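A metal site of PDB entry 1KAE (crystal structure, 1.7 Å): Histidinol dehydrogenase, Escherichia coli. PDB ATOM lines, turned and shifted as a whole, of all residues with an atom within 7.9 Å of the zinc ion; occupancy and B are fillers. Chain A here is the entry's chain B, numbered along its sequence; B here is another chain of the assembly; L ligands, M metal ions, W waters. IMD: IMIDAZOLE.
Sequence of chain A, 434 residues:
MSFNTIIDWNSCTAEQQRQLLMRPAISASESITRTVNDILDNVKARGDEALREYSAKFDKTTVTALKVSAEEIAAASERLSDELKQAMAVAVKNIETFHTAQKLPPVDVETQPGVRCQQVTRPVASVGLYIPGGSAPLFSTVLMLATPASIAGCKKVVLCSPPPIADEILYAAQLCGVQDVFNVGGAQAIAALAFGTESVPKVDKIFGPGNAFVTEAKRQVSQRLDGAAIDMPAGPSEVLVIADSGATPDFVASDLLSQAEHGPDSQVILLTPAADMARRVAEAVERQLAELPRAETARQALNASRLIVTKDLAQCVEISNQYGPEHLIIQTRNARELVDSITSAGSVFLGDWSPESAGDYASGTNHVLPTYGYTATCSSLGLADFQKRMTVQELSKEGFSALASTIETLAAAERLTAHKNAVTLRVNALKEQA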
ATOM      1  N   LEU A 138      -7.805 -26.907 -23.352  1.00  0.00           N
ATOM      2  CA  LEU A 138      -6.706 -27.443 -22.558  1.00  0.00           C
ATOM      3  C   LEU A 138      -7.195 -28.784 -22.009  1.00  0.00           C
ATOM      4  O   LEU A 138      -7.527 -28.924 -20.818  1.00  0.00           O
ATOM      5  CB  LEU A 138      -6.341 -26.450 -21.437  1.00  0.00           C
ATOM      6  CG  LEU A 138      -5.989 -25.010 -21.879  1.00  0.00           C
ATOM      7  CD1 LEU A 138      -5.272 -24.218 -20.738  1.00  0.00           C
ATOM      8  CD2 LEU A 138      -5.096 -25.077 -23.108  1.00  0.00           C
ATOM      9  N   SER A 140      -5.642 -31.277 -21.209  1.00  0.00           N
ATOM     10  CA  SER A 140      -4.805 -31.896 -20.187  1.00  0.00           C
ATOM     11  C   SER A 140      -5.473 -31.761 -18.808  1.00  0.00           C
ATOM     12  O   SER A 140      -5.270 -32.579 -17.938  1.00  0.00           O
ATOM     13  CB  SER A 140      -3.403 -31.289 -20.179  1.00  0.00           C
ATOM     14  OG  SER A 140      -3.440 -29.902 -19.907  1.00  0.00           O
ATOM     15  N   SER A 237      -3.415 -16.773 -12.740  1.00  0.00           N
ATOM     16  CA  SER A 237      -2.295 -17.654 -12.512  1.00  0.00           C
ATOM     17  C   SER A 237      -0.953 -16.915 -12.392  1.00  0.00           C
ATOM     18  O   SER A 237      -0.842 -15.721 -12.691  1.00  0.00           O
ATOM     19  CB  SER A 237      -2.213 -18.671 -13.636  1.00  0.00           C
ATOM     20  OG  SER A 237      -2.678 -18.069 -14.812  1.00  0.00           O
ATOM     21  N   SER A 258       5.999 -19.128 -20.898  1.00  0.00           N
ATOM     22  CA  SER A 258       4.965 -20.209 -20.903  1.00  0.00           C
ATOM     23  C   SER A 258       3.796 -19.774 -20.063  1.00  0.00           C
ATOM     24  O   SER A 258       2.646 -19.960 -20.412  1.00  0.00           O
ATOM     25  CB  SER A 258       5.493 -21.574 -20.373  1.00  0.00           C
ATOM     26  OG  SER A 258       6.330 -21.456 -19.224  1.00  0.00           O
ATOM     27  N   GLN A 259       4.079 -19.174 -18.923  1.00  0.00           N
ATOM     28  CA  GLN A 259       2.970 -18.730 -18.095  1.00  0.00           C
ATOM     29  C   GLN A 259       2.268 -17.472 -18.675  1.00  0.00           C
ATOM     30  O   GLN A 259       1.039 -17.340 -18.594  1.00  0.00           O
ATOM     31  CB  GLN A 259       3.526 -18.449 -16.713  1.00  0.00           C
ATOM     32  CG  GLN A 259       2.622 -17.673 -15.761  1.00  0.00           C
ATOM     33  CD  GLN A 259       1.533 -18.528 -15.173  1.00  0.00           C
ATOM     34  OE1 GLN A 259       1.763 -19.706 -14.826  1.00  0.00           O
ATOM     35  NE2 GLN A 259       0.326 -17.943 -15.012  1.00  0.00           N
ATOM     36  N   ALA A 260       3.022 -16.540 -19.252  1.00  0.00           N
ATOM     37  CA  ALA A 260       2.414 -15.302 -19.782  1.00  0.00           C
ATOM     38  C   ALA A 260       1.410 -15.579 -20.877  1.00  0.00           C
ATOM     39  O   ALA A 260       0.360 -14.914 -20.955  1.00  0.00           O
ATOM     40  CB  ALA A 260       3.503 -14.355 -20.291  1.00  0.00           C
ATOM     41  N   GLU A 261       1.674 -16.610 -21.690  1.00  0.00           N
ATOM     42  CA  GLU A 261       0.759 -16.941 -22.801  1.00  0.00           C
ATOM     43  C   GLU A 261      -0.581 -17.525 -22.398  1.00  0.00           C
ATOM     44  O   GLU A 261      -1.484 -17.637 -23.232  1.00  0.00           O
ATOM     45  CB  GLU A 261       1.447 -17.886 -23.820  1.00  0.00           C
ATOM     46  CG  GLU A 261       1.451 -19.360 -23.423  1.00  0.00           C
ATOM     47  CD  GLU A 261       1.994 -20.229 -24.549  1.00  0.00           C
ATOM     48  OE1 GLU A 261       2.233 -19.716 -25.679  1.00  0.00           O
ATOM     49  OE2 GLU A 261       2.188 -21.434 -24.330  1.00  0.00           O
ATOM     50  N   HIS A 262      -0.738 -17.890 -21.130  1.00  0.00           N
ATOM     51  CA  HIS A 262      -1.996 -18.455 -20.679  1.00  0.00           C
ATOM     52  C   HIS A 262      -3.142 -17.435 -20.730  1.00  0.00           C
ATOM     53  O   HIS A 262      -4.253 -17.801 -21.117  1.00  0.00           O
ATOM     54  CB  HIS A 262      -1.892 -18.982 -19.238  1.00  0.00           C
ATOM     55  CG  HIS A 262      -1.451 -20.412 -19.150  1.00  0.00           C
ATOM     56  ND1 HIS A 262      -2.163 -21.448 -19.732  1.00  0.00           N
ATOM     57  CD2 HIS A 262      -0.409 -20.990 -18.502  1.00  0.00           C
ATOM     58  CE1 HIS A 262      -1.571 -22.601 -19.445  1.00  0.00           C
ATOM     59  NE2 HIS A 262      -0.503 -22.349 -18.699  1.00  0.00           N
ATOM     60  N   HIS A 327       3.250 -21.187  -9.025  1.00  0.00           N
ATOM     61  CA  HIS A 327       4.352 -22.056  -9.465  1.00  0.00           C
ATOM     62  C   HIS A 327       5.635 -21.359  -9.071  1.00  0.00           C
ATOM     63  O   HIS A 327       5.783 -20.149  -9.326  1.00  0.00           O
ATOM     64  CB  HIS A 327       4.402 -22.210 -11.013  1.00  0.00           C
ATOM     65  CG  HIS A 327       3.135 -22.745 -11.637  1.00  0.00           C
ATOM     66  ND1 HIS A 327       2.120 -21.927 -12.086  1.00  0.00           N
ATOM     67  CD2 HIS A 327       2.750 -24.007 -11.945  1.00  0.00           C
ATOM     68  CE1 HIS A 327       1.168 -22.654 -12.638  1.00  0.00           C
ATOM     69  NE2 HIS A 327       1.526 -23.924 -12.558  1.00  0.00           N
ATOM     70  N   GLU A 356       8.167 -25.388 -16.440  1.00  0.00           N
ATOM     71  CA  GLU A 356       6.810 -25.495 -15.958  1.00  0.00           C
ATOM     72  C   GLU A 356       6.029 -26.453 -16.865  1.00  0.00           C
ATOM     73  O   GLU A 356       5.168 -27.202 -16.378  1.00  0.00           O
ATOM     74  CB  GLU A 356       6.110 -24.127 -15.934  1.00  0.00           C
ATOM     75  CG  GLU A 356       4.667 -24.236 -15.448  1.00  0.00           C
ATOM     76  CD  GLU A 356       4.142 -22.901 -14.958  1.00  0.00           C
ATOM     77  OE1 GLU A 356       4.970 -22.083 -14.495  1.00  0.00           O
ATOM     78  OE2 GLU A 356       2.915 -22.659 -15.008  1.00  0.00           O
ATOM     79  N   SER A 357       6.324 -26.421 -18.178  1.00  0.00           N
ATOM     80  CA  SER A 357       5.661 -27.310 -19.158  1.00  0.00           C
ATOM     81  C   SER A 357       5.712 -28.764 -18.724  1.00  0.00           C
ATOM     82  O   SER A 357       4.743 -29.509 -18.913  1.00  0.00           O
ATOM     83  CB  SER A 357       6.332 -27.216 -20.567  1.00  0.00           C
ATOM     84  OG  SER A 357       6.544 -25.874 -20.890  1.00  0.00           O
ATOM     85  N   GLY A 359       5.636 -29.992 -15.742  1.00  0.00           N
ATOM     86  CA  GLY A 359       4.607 -30.227 -14.708  1.00  0.00           C
ATOM     87  C   GLY A 359       3.163 -30.060 -15.231  1.00  0.00           C
ATOM     88  O   GLY A 359       2.247 -30.808 -14.835  1.00  0.00           O
ATOM     89  N   ASP A 360       2.970 -29.075 -16.111  1.00  0.00           N
ATOM     90  CA  ASP A 360       1.678 -28.796 -16.706  1.00  0.00           C
ATOM     91  C   ASP A 360       1.153 -30.034 -17.427  1.00  0.00           C
ATOM     92  O   ASP A 360      -0.006 -30.341 -17.363  1.00  0.00           O
ATOM     93  CB  ASP A 360       1.772 -27.659 -17.761  1.00  0.00           C
ATOM     94  CG  ASP A 360       1.890 -26.276 -17.155  1.00  0.00           C
ATOM     95  OD1 ASP A 360       1.737 -26.088 -15.934  1.00  0.00           O
ATOM     96  OD2 ASP A 360       2.157 -25.324 -17.920  1.00  0.00           O
ATOM     97  N   TYR A 361       2.055 -30.799 -18.043  1.00  0.00           N
ATOM     98  CA  TYR A 361       1.671 -31.957 -18.851  1.00  0.00           C
ATOM     99  C   TYR A 361       2.002 -33.374 -18.471  1.00  0.00           C
ATOM    100  O   TYR A 361       1.146 -34.246 -18.619  1.00  0.00           O
ATOM    101  CB  TYR A 361       2.236 -31.773 -20.258  1.00  0.00           C
ATOM    102  CG  TYR A 361       1.646 -30.611 -20.986  1.00  0.00           C
ATOM    103  CD1 TYR A 361       2.407 -29.469 -21.256  1.00  0.00           C
ATOM    104  CD2 TYR A 361       0.304 -30.635 -21.390  1.00  0.00           C
ATOM    105  CE1 TYR A 361       1.833 -28.370 -21.918  1.00  0.00           C
ATOM    106  CE2 TYR A 361      -0.264 -29.567 -22.052  1.00  0.00           C
ATOM    107  CZ  TYR A 361       0.490 -28.431 -22.324  1.00  0.00           C
ATOM    108  OH  TYR A 361      -0.108 -27.365 -22.964  1.00  0.00           O
ATOM    109  N   HIS A 367      -1.506 -29.984 -12.089  1.00  0.00           N
ATOM    110  CA  HIS A 367      -1.326 -28.590 -12.483  1.00  0.00           C
ATOM    111  C   HIS A 367      -2.466 -27.688 -11.991  1.00  0.00           C
ATOM    112  O   HIS A 367      -2.428 -26.455 -12.217  1.00  0.00           O
ATOM    113  CB  HIS A 367      -1.082 -28.468 -14.019  1.00  0.00           C
ATOM    114  CG  HIS A 367      -2.299 -28.684 -14.896  1.00  0.00           C
ATOM    115  ND1 HIS A 367      -2.177 -29.210 -16.163  1.00  0.00           N
ATOM    116  CD2 HIS A 367      -3.593 -28.326 -14.751  1.00  0.00           C
ATOM    117  CE1 HIS A 367      -3.357 -29.160 -16.775  1.00  0.00           C
ATOM    118  NE2 HIS A 367      -4.228 -28.635 -15.928  1.00  0.00           N
ATOM    119  N   GLU B 414      -2.500 -28.352 -27.592  1.00  0.00           N
ATOM    120  CA  GLU B 414      -3.270 -27.304 -26.910  1.00  0.00           C
ATOM    121  C   GLU B 414      -2.933 -25.925 -27.475  1.00  0.00           C
ATOM    122  O   GLU B 414      -3.366 -24.915 -26.949  1.00  0.00           O
ATOM    123  CB  GLU B 414      -2.979 -27.298 -25.406  1.00  0.00           C
ATOM    124  CG  GLU B 414      -3.337 -28.596 -24.676  1.00  0.00           C
ATOM    125  CD  GLU B 414      -3.348 -28.439 -23.178  1.00  0.00           C
ATOM    126  OE1 GLU B 414      -2.582 -27.623 -22.641  1.00  0.00           O
ATOM    127  OE2 GLU B 414      -4.124 -29.114 -22.502  1.00  0.00           O
ATOM    128  N   LEU B 416      -0.187 -24.206 -27.350  1.00  0.00           N
ATOM    129  CA  LEU B 416       0.537 -23.356 -26.404  1.00  0.00           C
ATOM    130  C   LEU B 416       2.008 -23.408 -26.824  1.00  0.00           C
ATOM    131  O   LEU B 416       2.813 -24.199 -26.315  1.00  0.00           O
ATOM    132  CB  LEU B 416       0.324 -23.859 -24.980  1.00  0.00           C
ATOM    133  CG  LEU B 416      -1.122 -23.569 -24.457  1.00  0.00           C
ATOM    134  CD1 LEU B 416      -1.342 -24.094 -23.079  1.00  0.00           C
ATOM    135  CD2 LEU B 416      -1.331 -22.034 -24.413  1.00  0.00           C
ATOM    136  N   HIS B 419       4.875 -22.909 -24.221  1.00  0.00           N
ATOM    137  CA  HIS B 419       5.058 -24.105 -23.395  1.00  0.00           C
ATOM    138  C   HIS B 419       5.914 -25.104 -24.163  1.00  0.00           C
ATOM    139  O   HIS B 419       6.797 -25.747 -23.580  1.00  0.00           O
ATOM    140  CB  HIS B 419       3.705 -24.796 -23.044  1.00  0.00           C
ATOM    141  CG  HIS B 419       2.941 -24.147 -21.916  1.00  0.00           C
ATOM    142  ND1 HIS B 419       2.351 -22.898 -22.029  1.00  0.00           N
ATOM    143  CD2 HIS B 419       2.610 -24.606 -20.686  1.00  0.00           C
ATOM    144  CE1 HIS B 419       1.684 -22.627 -20.928  1.00  0.00           C
ATOM    145  NE2 HIS B 419       1.821 -23.638 -20.088  1.00  0.00           N
HETATM  146  N1  IMD L   1      -1.899 -26.706 -20.053  1.00  0.00           N
HETATM  147  C2  IMD L   1      -0.817 -25.935 -20.057  1.00  0.00           C
HETATM  148  N3  IMD L   1      -0.661 -25.409 -18.846  1.00  0.00           N
HETATM  149  C4  IMD L   1      -1.687 -25.860 -18.031  1.00  0.00           C
HETATM  150  C5  IMD L   1      -2.467 -26.659 -18.804  1.00  0.00           C
HETATM  151 ZN    ZN M   1       0.756 -23.962 -18.375  1.00  0.00          ZN
HETATM  152  O   HOH W   1       0.651 -23.675 -16.313  1.00  0.00           O
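The zinc ion is bound by OD2 of Asp 360 (2.0 Å). NE2 of His 419 of chain B binds the zinc ion (2.0 Å). The zinc ion is bound by a ring nitrogen (NE2) of His 262. N3 of the ligand is bound to the zinc ion (2.1 Å). Water W1 binds the zinc ion, 2.1 Å away. The zinc ion has five donor atoms within binding distance.
O of Asp 360 sits at hydrogen-bond distance from ND1 of His 367 (2.7 Å). The backbone carbonyl oxygen of Ser 258 sits close to a ring nitrogen (ND1) of His 419 of chain B (3.4 Å). The backbone carbonyl oxygen of His 419 of chain B lies within hydrogen-bond range of the side-chain hydroxyl of Ser 357 (2.7 Å). The side-chain carboxylate (OE2) of Glu 261 is in hydrogen-bond range of a ring nitrogen (ND1) of His 419 of chain B (2.7 Å).
Water W1 lies within hydrogen-bond range of the side-chain carboxylate of Asp 360 (2.7 Å) and the side-chain carboxylate of Glu 356 (2.8 Å).
Three residues have an atom within 4 Å of the zinc ion: His 262, Asp 360 and His 419 of chain B. The nearest printed residue that does not touch the zinc ion is Glu 356 (4.2 Å).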
